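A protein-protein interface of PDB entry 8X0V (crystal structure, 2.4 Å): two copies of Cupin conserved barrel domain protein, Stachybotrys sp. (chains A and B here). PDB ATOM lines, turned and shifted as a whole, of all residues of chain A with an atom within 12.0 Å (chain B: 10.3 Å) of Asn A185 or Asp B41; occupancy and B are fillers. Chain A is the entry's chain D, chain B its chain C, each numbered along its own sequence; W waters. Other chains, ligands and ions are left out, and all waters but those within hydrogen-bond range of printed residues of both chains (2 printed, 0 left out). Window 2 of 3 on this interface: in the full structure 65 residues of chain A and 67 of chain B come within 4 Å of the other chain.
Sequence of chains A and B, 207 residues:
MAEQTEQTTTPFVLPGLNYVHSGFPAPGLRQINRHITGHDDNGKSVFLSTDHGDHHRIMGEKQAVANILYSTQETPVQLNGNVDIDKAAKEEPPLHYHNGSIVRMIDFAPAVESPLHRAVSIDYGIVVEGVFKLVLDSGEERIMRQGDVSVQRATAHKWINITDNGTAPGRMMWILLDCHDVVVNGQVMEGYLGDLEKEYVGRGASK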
ATOM      1  N   ARG A 118       9.066  21.157 -20.579  1.00  0.00           N
ATOM      2  CA  ARG A 118       9.084  21.607 -19.194  1.00  0.00           C
ATOM      3  C   ARG A 118       9.790  22.947 -19.114  1.00  0.00           C
ATOM      4  O   ARG A 118      10.952  23.066 -19.517  1.00  0.00           O
ATOM      5  CB  ARG A 118       9.775  20.598 -18.276  1.00  0.00           C
ATOM      6  CG  ARG A 118       9.820  21.057 -16.825  1.00  0.00           C
ATOM      7  CD  ARG A 118      10.937  20.384 -16.051  1.00  0.00           C
ATOM      8  NE  ARG A 118      10.916  18.936 -16.213  1.00  0.00           N
ATOM      9  CZ  ARG A 118      10.091  18.128 -15.555  1.00  0.00           C
ATOM     10  NH1 ARG A 118       9.217  18.631 -14.696  1.00  0.00           N
ATOM     11  NH2 ARG A 118      10.139  16.818 -15.760  1.00  0.00           N
ATOM     12  N   ASP A 137       3.483  14.306 -18.774  1.00  0.00           N
ATOM     13  CA  ASP A 137       4.348  13.255 -19.298  1.00  0.00           C
ATOM     14  C   ASP A 137       4.010  11.884 -18.722  1.00  0.00           C
ATOM     15  O   ASP A 137       4.365  10.867 -19.326  1.00  0.00           O
ATOM     16  CB  ASP A 137       5.823  13.605 -19.056  1.00  0.00           C
ATOM     17  CG  ASP A 137       6.234  13.515 -17.592  1.00  0.00           C
ATOM     18  OD1 ASP A 137       5.361  13.371 -16.712  1.00  0.00           O
ATOM     19  OD2 ASP A 137       7.454  13.596 -17.325  1.00  0.00           O
ATOM     20  N   SER A 138       3.326  11.837 -17.578  1.00  0.00           N
ATOM     21  CA  SER A 138       2.820  10.578 -17.043  1.00  0.00           C
ATOM     22  C   SER A 138       1.668  10.010 -17.861  1.00  0.00           C
ATOM     23  O   SER A 138       1.257   8.872 -17.613  1.00  0.00           O
ATOM     24  CB  SER A 138       2.362  10.767 -15.597  1.00  0.00           C
ATOM     25  OG  SER A 138       1.239  11.633 -15.533  1.00  0.00           O
ATOM     26  N   GLU A 140      -1.354  11.264 -17.694  1.00  0.00           N
ATOM     27  CA  GLU A 140      -2.544  11.855 -17.098  1.00  0.00           C
ATOM     28  C   GLU A 140      -2.949  13.102 -17.872  1.00  0.00           C
ATOM     29  O   GLU A 140      -2.106  13.830 -18.405  1.00  0.00           O
ATOM     30  CB  GLU A 140      -2.291  12.215 -15.635  1.00  0.00           C
ATOM     31  CG  GLU A 140      -2.075  11.031 -14.707  1.00  0.00           C
ATOM     32  CD  GLU A 140      -2.044  11.445 -13.242  1.00  0.00           C
ATOM     33  OE1 GLU A 140      -1.426  10.731 -12.426  1.00  0.00           O
ATOM     34  OE2 GLU A 140      -2.636  12.490 -12.903  1.00  0.00           O
ATOM     35  N   ARG A 153       3.197  23.432 -11.809  1.00  0.00           N
ATOM     36  CA  ARG A 153       4.322  23.546 -10.882  1.00  0.00           C
ATOM     37  C   ARG A 153       5.569  22.894 -11.484  1.00  0.00           C
ATOM     38  O   ARG A 153       6.045  21.848 -11.040  1.00  0.00           O
ATOM     39  CB  ARG A 153       3.951  22.943  -9.531  1.00  0.00           C
ATOM     40  CG  ARG A 153       2.767  23.650  -8.879  1.00  0.00           C
ATOM     41  CD  ARG A 153       2.359  23.011  -7.564  1.00  0.00           C
ATOM     42  NE  ARG A 153       3.476  22.889  -6.634  1.00  0.00           N
ATOM     43  CZ  ARG A 153       4.038  21.732  -6.293  1.00  0.00           C
ATOM     44  NH1 ARG A 153       3.582  20.597  -6.807  1.00  0.00           N
ATOM     45  NH2 ARG A 153       5.051  21.711  -5.437  1.00  0.00           N
ATOM     46  N   THR A 155       6.106  21.271 -14.124  1.00  0.00           N
ATOM     47  CA  THR A 155       5.917  19.914 -14.606  1.00  0.00           C
ATOM     48  C   THR A 155       6.021  19.868 -16.131  1.00  0.00           C
ATOM     49  O   THR A 155       5.882  20.883 -16.822  1.00  0.00           O
ATOM     50  CB  THR A 155       4.562  19.377 -14.148  1.00  0.00           C
ATOM     51  OG1 THR A 155       3.572  20.404 -14.282  1.00  0.00           O
ATOM     52  CG2 THR A 155       4.623  18.947 -12.690  1.00  0.00           C
ATOM     53  N   ASP A 181      14.246  25.264  -8.843  1.00  0.00           N
ATOM     54  CA  ASP A 181      14.128  24.039  -9.621  1.00  0.00           C
ATOM     55  C   ASP A 181      13.677  22.879  -8.743  1.00  0.00           C
ATOM     56  O   ASP A 181      14.053  22.776  -7.571  1.00  0.00           O
ATOM     57  CB  ASP A 181      15.452  23.707 -10.304  1.00  0.00           C
ATOM     58  CG  ASP A 181      15.262  23.266 -11.742  1.00  0.00           C
ATOM     59  OD1 ASP A 181      14.330  22.470 -11.996  1.00  0.00           O
ATOM     60  OD2 ASP A 181      16.025  23.728 -12.617  1.00  0.00           O
ATOM     61  N   VAL A 182      12.864  22.005  -9.327  1.00  0.00           N
ATOM     62  CA  VAL A 182      12.258  20.901  -8.593  1.00  0.00           C
ATOM     63  C   VAL A 182      13.239  19.745  -8.527  1.00  0.00           C
ATOM     64  O   VAL A 182      13.759  19.295  -9.554  1.00  0.00           O
ATOM     65  CB  VAL A 182      10.941  20.468  -9.256  1.00  0.00           C
ATOM     66  CG1 VAL A 182      10.243  19.416  -8.407  1.00  0.00           C
ATOM     67  CG2 VAL A 182      10.045  21.667  -9.469  1.00  0.00           C
ATOM     68  N   VAL A 183      13.474  19.242  -7.320  1.00  0.00           N
ATOM     69  CA  VAL A 183      14.438  18.176  -7.077  1.00  0.00           C
ATOM     70  C   VAL A 183      13.679  16.949  -6.595  1.00  0.00           C
ATOM     71  O   VAL A 183      13.013  16.993  -5.552  1.00  0.00           O
ATOM     72  CB  VAL A 183      15.507  18.600  -6.059  1.00  0.00           C
ATOM     73  CG1 VAL A 183      16.328  17.401  -5.624  1.00  0.00           C
ATOM     74  CG2 VAL A 183      16.395  19.689  -6.653  1.00  0.00           C
ATOM     75  N   VAL A 184      13.780  15.856  -7.351  1.00  0.00           N
ATOM     76  CA  VAL A 184      13.122  14.595  -7.028  1.00  0.00           C
ATOM     77  C   VAL A 184      14.180  13.502  -6.975  1.00  0.00           C
ATOM     78  O   VAL A 184      14.971  13.353  -7.914  1.00  0.00           O
ATOM     79  CB  VAL A 184      12.030  14.244  -8.058  1.00  0.00           C
ATOM     80  CG1 VAL A 184      11.476  12.849  -7.794  1.00  0.00           C
ATOM     81  CG2 VAL A 184      10.914  15.281  -8.030  1.00  0.00           C
ATOM     82  N   ASN A 185      14.190  12.742  -5.876  1.00  0.00           N
ATOM     83  CA  ASN A 185      15.149  11.653  -5.677  1.00  0.00           C
ATOM     84  C   ASN A 185      16.589  12.148  -5.786  1.00  0.00           C
ATOM     85  O   ASN A 185      17.485  11.401  -6.187  1.00  0.00           O
ATOM     86  CB  ASN A 185      14.906  10.508  -6.665  1.00  0.00           C
ATOM     87  CG  ASN A 185      13.801   9.575  -6.216  1.00  0.00           C
ATOM     88  OD1 ASN A 185      13.109   9.841  -5.232  1.00  0.00           O
ATOM     89  ND2 ASN A 185      13.628   8.473  -6.937  1.00  0.00           N
ATOM     90  N   GLY A 186      16.820  13.410  -5.431  1.00  0.00           N
ATOM     91  CA  GLY A 186      18.120  14.018  -5.619  1.00  0.00           C
ATOM     92  C   GLY A 186      18.458  14.373  -7.048  1.00  0.00           C
ATOM     93  O   GLY A 186      19.596  14.763  -7.321  1.00  0.00           O
ATOM     94  N   GLN A 187      17.506  14.255  -7.970  1.00  0.00           N
ATOM     95  CA  GLN A 187      17.736  14.506  -9.386  1.00  0.00           C
ATOM     96  C   GLN A 187      17.082  15.824  -9.776  1.00  0.00           C
ATOM     97  O   GLN A 187      15.872  15.997  -9.598  1.00  0.00           O
ATOM     98  CB  GLN A 187      17.188  13.363 -10.242  1.00  0.00           C
ATOM     99  CG  GLN A 187      17.822  13.271 -11.621  1.00  0.00           C
ATOM    100  CD  GLN A 187      17.365  12.051 -12.399  1.00  0.00           C
ATOM    101  OE1 GLN A 187      16.241  11.577 -12.229  1.00  0.00           O
ATOM    102  NE2 GLN A 187      18.238  11.538 -13.259  1.00  0.00           N
ATOM    103  N   VAL A 188      17.884  16.749 -10.299  1.00  0.00           N
ATOM    104  CA  VAL A 188      17.330  17.973 -10.862  1.00  0.00           C
ATOM    105  C   VAL A 188      16.465  17.611 -12.063  1.00  0.00           C
ATOM    106  O   VAL A 188      16.943  17.024 -13.041  1.00  0.00           O
ATOM    107  CB  VAL A 188      18.448  18.958 -11.230  1.00  0.00           C
ATOM    108  CG1 VAL A 188      19.563  18.261 -12.013  1.00  0.00           C
ATOM    109  CG2 VAL A 188      17.884  20.133 -12.015  1.00  0.00           C
ATOM    110  N   MET A 189      15.178  17.936 -11.984  1.00  0.00           N
ATOM    111  CA  MET A 189      14.258  17.680 -13.090  1.00  0.00           C
ATOM    112  C   MET A 189      14.458  18.779 -14.125  1.00  0.00           C
ATOM    113  O   MET A 189      13.916  19.877 -13.997  1.00  0.00           O
ATOM    114  CB  MET A 189      12.818  17.615 -12.594  1.00  0.00           C
ATOM    115  CG  MET A 189      12.548  16.387 -11.742  1.00  0.00           C
ATOM    116  SD  MET A 189      13.183  14.928 -12.598  1.00  0.00           S
ATOM    117  CE  MET A 189      11.771  13.835 -12.610  1.00  0.00           C
ATOM    118  N   GLU A 190      15.236  18.475 -15.160  1.00  0.00           N
ATOM    119  CA  GLU A 190      15.748  19.499 -16.058  1.00  0.00           C
ATOM    120  C   GLU A 190      14.674  19.967 -17.034  1.00  0.00           C
ATOM    121  O   GLU A 190      13.959  19.152 -17.626  1.00  0.00           O
ATOM    122  CB  GLU A 190      16.960  18.974 -16.827  1.00  0.00           C
ATOM    123  CG  GLU A 190      17.915  20.064 -17.284  1.00  0.00           C
ATOM    124  CD  GLU A 190      18.969  19.553 -18.246  1.00  0.00           C
ATOM    125  OE1 GLU A 190      18.662  18.628 -19.029  1.00  0.00           O
ATOM    126  OE2 GLU A 190      20.103  20.078 -18.215  1.00  0.00           O
ATOM    127  N   GLY B  38       1.947  18.337 -10.118  1.00  0.00           N
ATOM    128  CA  GLY B  38       3.082  18.065  -9.266  1.00  0.00           C
ATOM    129  C   GLY B  38       3.898  16.898  -9.780  1.00  0.00           C
ATOM    130  O   GLY B  38       3.699  16.420 -10.898  1.00  0.00           O
ATOM    131  N   HIS B  39       4.821  16.439  -8.934  1.00  0.00           N
ATOM    132  CA  HIS B  39       5.735  15.350  -9.257  1.00  0.00           C
ATOM    133  C   HIS B  39       5.532  14.188  -8.293  1.00  0.00           C
ATOM    134  O   HIS B  39       5.369  14.394  -7.087  1.00  0.00           O
ATOM    135  CB  HIS B  39       7.191  15.816  -9.198  1.00  0.00           C
ATOM    136  CG  HIS B  39       7.592  16.702 -10.336  1.00  0.00           C
ATOM    137  ND1 HIS B  39       7.411  18.069 -10.316  1.00  0.00           N
ATOM    138  CD2 HIS B  39       8.177  16.418 -11.524  1.00  0.00           C
ATOM    139  CE1 HIS B  39       7.862  18.586 -11.445  1.00  0.00           C
ATOM    140  NE2 HIS B  39       8.333  17.605 -12.195  1.00  0.00           N
ATOM    141  N   ASP B  40       5.548  12.967  -8.828  1.00  0.00           N
ATOM    142  CA  ASP B  40       5.330  11.770  -8.026  1.00  0.00           C
ATOM    143  C   ASP B  40       6.667  11.168  -7.583  1.00  0.00           C
ATOM    144  O   ASP B  40       7.722  11.802  -7.672  1.00  0.00           O
ATOM    145  CB  ASP B  40       4.460  10.769  -8.792  1.00  0.00           C
ATOM    146  CG  ASP B  40       5.174  10.135  -9.977  1.00  0.00           C
ATOM    147  OD1 ASP B  40       6.304  10.547 -10.316  1.00  0.00           O
ATOM    148  OD2 ASP B  40       4.590   9.210 -10.579  1.00  0.00           O
ATOM    149  N   ASP B  41       6.623   9.922  -7.093  1.00  0.00           N
ATOM    150  CA  ASP B  41       7.796   9.294  -6.494  1.00  0.00           C
ATOM    151  C   ASP B  41       8.936   9.117  -7.486  1.00  0.00           C
ATOM    152  O   ASP B  41      10.105   9.075  -7.085  1.00  0.00           O
ATOM    153  CB  ASP B  41       7.419   7.932  -5.910  1.00  0.00           C
ATOM    154  CG  ASP B  41       6.478   8.039  -4.731  1.00  0.00           C
ATOM    155  OD1 ASP B  41       5.876   9.118  -4.543  1.00  0.00           O
ATOM    156  OD2 ASP B  41       6.343   7.043  -3.988  1.00  0.00           O
ATOM    157  N   ASN B  42       8.625   8.991  -8.776  1.00  0.00           N
ATOM    158  CA  ASN B  42       9.630   8.681  -9.785  1.00  0.00           C
ATOM    159  C   ASN B  42       9.844   9.836 -10.753  1.00  0.00           C
ATOM    160  O   ASN B  42      10.390   9.639 -11.846  1.00  0.00           O
ATOM    161  CB  ASN B  42       9.240   7.406 -10.533  1.00  0.00           C
ATOM    162  CG  ASN B  42       8.913   6.267  -9.587  1.00  0.00           C
ATOM    163  OD1 ASN B  42       7.780   5.787  -9.543  1.00  0.00           O
ATOM    164  ND2 ASN B  42       9.903   5.843  -8.808  1.00  0.00           N
ATOM    165  N   GLY B  43       9.433  11.040 -10.364  1.00  0.00           N
ATOM    166  CA  GLY B  43       9.659  12.221 -11.166  1.00  0.00           C
ATOM    167  C   GLY B  43       8.687  12.425 -12.302  1.00  0.00           C
ATOM    168  O   GLY B  43       8.871  13.364 -13.085  1.00  0.00           O
ATOM    169  N   LYS B  44       7.672  11.574 -12.430  1.00  0.00           N
ATOM    170  CA  LYS B  44       6.650  11.766 -13.444  1.00  0.00           C
ATOM    171  C   LYS B  44       5.728  12.911 -13.047  1.00  0.00           C
ATOM    172  O   LYS B  44       5.374  13.069 -11.874  1.00  0.00           O
ATOM    173  CB  LYS B  44       5.850  10.480 -13.650  1.00  0.00           C
ATOM    174  CG  LYS B  44       6.709   9.268 -13.980  1.00  0.00           C
ATOM    175  CD  LYS B  44       6.228   8.564 -15.235  1.00  0.00           C
ATOM    176  CE  LYS B  44       7.394   8.093 -16.091  1.00  0.00           C
ATOM    177  NZ  LYS B  44       6.974   7.054 -17.076  1.00  0.00           N
ATOM    178  N   SER B  45       5.351  13.718 -14.032  1.00  0.00           N
ATOM    179  CA  SER B  45       4.474  14.857 -13.800  1.00  0.00           C
ATOM    180  C   SER B  45       3.028  14.377 -13.749  1.00  0.00           C
ATOM    181  O   SER B  45       2.536  13.779 -14.709  1.00  0.00           O
ATOM    182  CB  SER B  45       4.661  15.899 -14.898  1.00  0.00           C
ATOM    183  OG  SER B  45       5.968  16.443 -14.870  1.00  0.00           O
ATOM    184  N   VAL B  46       2.344  14.644 -12.637  1.00  0.00           N
ATOM    185  CA  VAL B  46       0.997  14.143 -12.411  1.00  0.00           C
ATOM    186  C   VAL B  46       0.118  15.278 -11.899  1.00  0.00           C
ATOM    187  O   VAL B  46       0.575  16.393 -11.647  1.00  0.00           O
ATOM    188  CB  VAL B  46       0.969  12.961 -11.424  1.00  0.00           C
ATOM    189  CG1 VAL B  46       1.670  11.749 -12.019  1.00  0.00           C
ATOM    190  CG2 VAL B  46       1.609  13.366 -10.106  1.00  0.00           C
ATOM    191  N   LEU B  48      -2.154  16.623  -8.886  1.00  0.00           N
ATOM    192  CA  LEU B  48      -2.288  16.431  -7.451  1.00  0.00           C
ATOM    193  C   LEU B  48      -3.698  16.700  -6.944  1.00  0.00           C
ATOM    194  O   LEU B  48      -4.092  16.141  -5.915  1.00  0.00           O
ATOM    195  CB  LEU B  48      -1.289  17.320  -6.706  1.00  0.00           C
ATOM    196  CG  LEU B  48       0.184  16.988  -6.959  1.00  0.00           C
ATOM    197  CD1 LEU B  48       1.093  17.987  -6.267  1.00  0.00           C
ATOM    198  CD2 LEU B  48       0.502  15.566  -6.509  1.00  0.00           C
ATOM    199  N   ASN B  80       9.796  22.407  -3.820  1.00  0.00           N
ATOM    200  CA  ASN B  80      10.243  21.116  -3.307  1.00  0.00           C
ATOM    201  C   ASN B  80       9.548  20.777  -1.996  1.00  0.00           C
ATOM    202  O   ASN B  80       9.272  21.653  -1.171  1.00  0.00           O
ATOM    203  CB  ASN B  80      11.756  21.120  -3.117  1.00  0.00           C
ATOM    204  CG  ASN B  80      12.501  21.115  -4.432  1.00  0.00           C
ATOM    205  OD1 ASN B  80      12.243  20.280  -5.299  1.00  0.00           O
ATOM    206  ND2 ASN B  80      13.425  22.056  -4.594  1.00  0.00           N
ATOM    207  N   GLY B  81       9.258  19.491  -1.811  1.00  0.00           N
ATOM    208  CA  GLY B  81       8.467  19.073  -0.673  1.00  0.00           C
ATOM    209  C   GLY B  81       7.033  19.547  -0.686  1.00  0.00           C
ATOM    210  O   GLY B  81       6.339  19.383   0.324  1.00  0.00           O
ATOM    211  N   ASN B  82       6.566  20.133  -1.794  1.00  0.00           N
ATOM    212  CA  ASN B  82       5.202  20.658  -1.913  1.00  0.00           C
ATOM    213  C   ASN B  82       4.881  21.663  -0.808  1.00  0.00           C
ATOM    214  O   ASN B  82       3.724  21.824  -0.416  1.00  0.00           O
ATOM    215  CB  ASN B  82       4.170  19.526  -1.919  1.00  0.00           C
ATOM    216  CG  ASN B  82       4.230  18.691  -3.185  1.00  0.00           C
ATOM    217  OD1 ASN B  82       4.735  19.139  -4.215  1.00  0.00           O
ATOM    218  ND2 ASN B  82       3.707  17.471  -3.116  1.00  0.00           N
HETATM  219  O   HOH W   1       5.254  18.310  -6.706  1.00  0.00           O
HETATM  220  O   HOH W   2       8.237  14.776 -14.966  1.00  0.00           O
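Of the printed residues of chain B, Thr A155 touches Gly B38 (3.2 Å), His B39 (3.5 Å) and Ser B45 (3.3 Å).
Of chain B, only His B39 (3.9 Å), Asp B40 (3.9 Å) and Gly B43 (3.7 Å) come within 4 Å of Val A184.
Asn A185 touches one residue of chain B.
Gln A187 touches none of the printed residues of chain B.
Val A188 touches none of the printed residues of chain B.
Of the printed residues of chain B, Met A189 touches Gly B43 (3.0 Å).
Of the printed residues of chain A, His B39 touches Arg A118 (2.8 Å), Arg A153 (3.8 Å), Thr A155 (3.5 Å), Val A182 (3.7 Å) and Val A184 (3.9 Å).
Asp B41 touches just one residue of chain A: Asn A185 (3.6 Å).
No residue of chain A comes within 4 Å of Asn B42.
Gly B43 touches two residues of chain A.
Printed residues of chain A within 4 Å of Val B46: Ser A138 (3.5 Å) and Glu A140 (3.3 Å).
Hydrophobic or aromatic side chains of chain B within 4 Å of the printed part of chain A: His B39, Val B46 and Leu B48.
Of the 16 printed residues of chain A, 12 touch a printed residue of chain B.
Hydrophobic or aromatic side chains of chain A that line the printed part of chain B: Val A182, Val A183, Val A184 and Met A189.
Among the printed residues, 23 pairs touch across the chains.
Among the printed residues, no Asp or Glu carboxylate lies within 4 Å of a Lys or Arg side-chain nitrogen of the other chain.
O of Asp A181 sits at hydrogen-bond distance from ND2 of Asn B80, at 3.1 Å.
O of Ser B45 lies within hydrogen-bond range of OG of Ser A138, at 2.6 Å.
A ring nitrogen (NE2) of His B39 lies within hydrogen-bond range of the guanidinium group (NH1) of Arg A118 (2.8 Å).
The backbone NH (N) of Ser B45 is in hydrogen-bond range of the side-chain carboxylate (OD1) of Asp A137, at 2.7 Å.
The backbone NH of Val A183 sits at hydrogen-bond distance from the side-chain amide oxygen of Asn B80, 2.6 Å away.
OD1 of Asn B82 sits at hydrogen-bond distance from NH2 of Arg A153 (2.9 Å).
Water W2 lies within hydrogen-bond range of O of Gly B43 (2.4 Å), OD2 of Asp A137 (2.8 Å), OG of Ser B45 (2.8 Å) and NH2 of Arg A118 (2.9 Å).
Water W1 lies within hydrogen-bond range of OD1 of Asn B82, NH1 of Arg A153 and N of His B39.
No position is printed for both chains.
Among the printed residues, pairs that only touch across the chains: Arg A118 with Ser B45 (3.9 Å), Asp A137 with Lys B44 (3.7 Å), Ser A138 with Val B46 (3.5 Å), Glu A140 with Val B46 (3.3 Å), Arg A153 with Gly B38 (3.6 Å), Arg A153 with His B39 (3.8 Å), Arg A153 with Leu B48 (3.6 Å), Thr A155 with Gly B38 (3.2 Å), Thr A155 with His B39 (3.5 Å), Thr A155 with Ser B45 (3.3 Å), Val A182 with His B39 (3.7 Å), Val A182 with Asn B80 (3.4 Å), Val A184 with His B39 (3.9 Å), Val A184 with Asp B40 (3.9 Å), Val A184 with Gly B43 (3.7 Å), Asn A185 with Asp B41 (3.6 Å) and Met A189 with Gly B43 (3.0 Å).
The side-chain carboxylate of Asp B40 lies within hydrogen-bond range of the backbone NH of Lys B44, at 2.7 Å.
The backbone NH (N) of Gly B38 sits at hydrogen-bond distance from the backbone carbonyl oxygen (O) of Val B46 (2.8 Å).
The backbone NH (N) of Asn B42 sits close to the side-chain carboxylate (OD1) of Asp B40 (3.2 Å).
The side-chain carboxylate of Asp B40 sits at hydrogen-bond distance from the backbone NH of Gly B43 (3.2 Å).
OG of Ser A138 lies close to N of Glu A140 (3.4 Å).
NE of Arg A118 lies within hydrogen-bond range of O of Glu A190.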
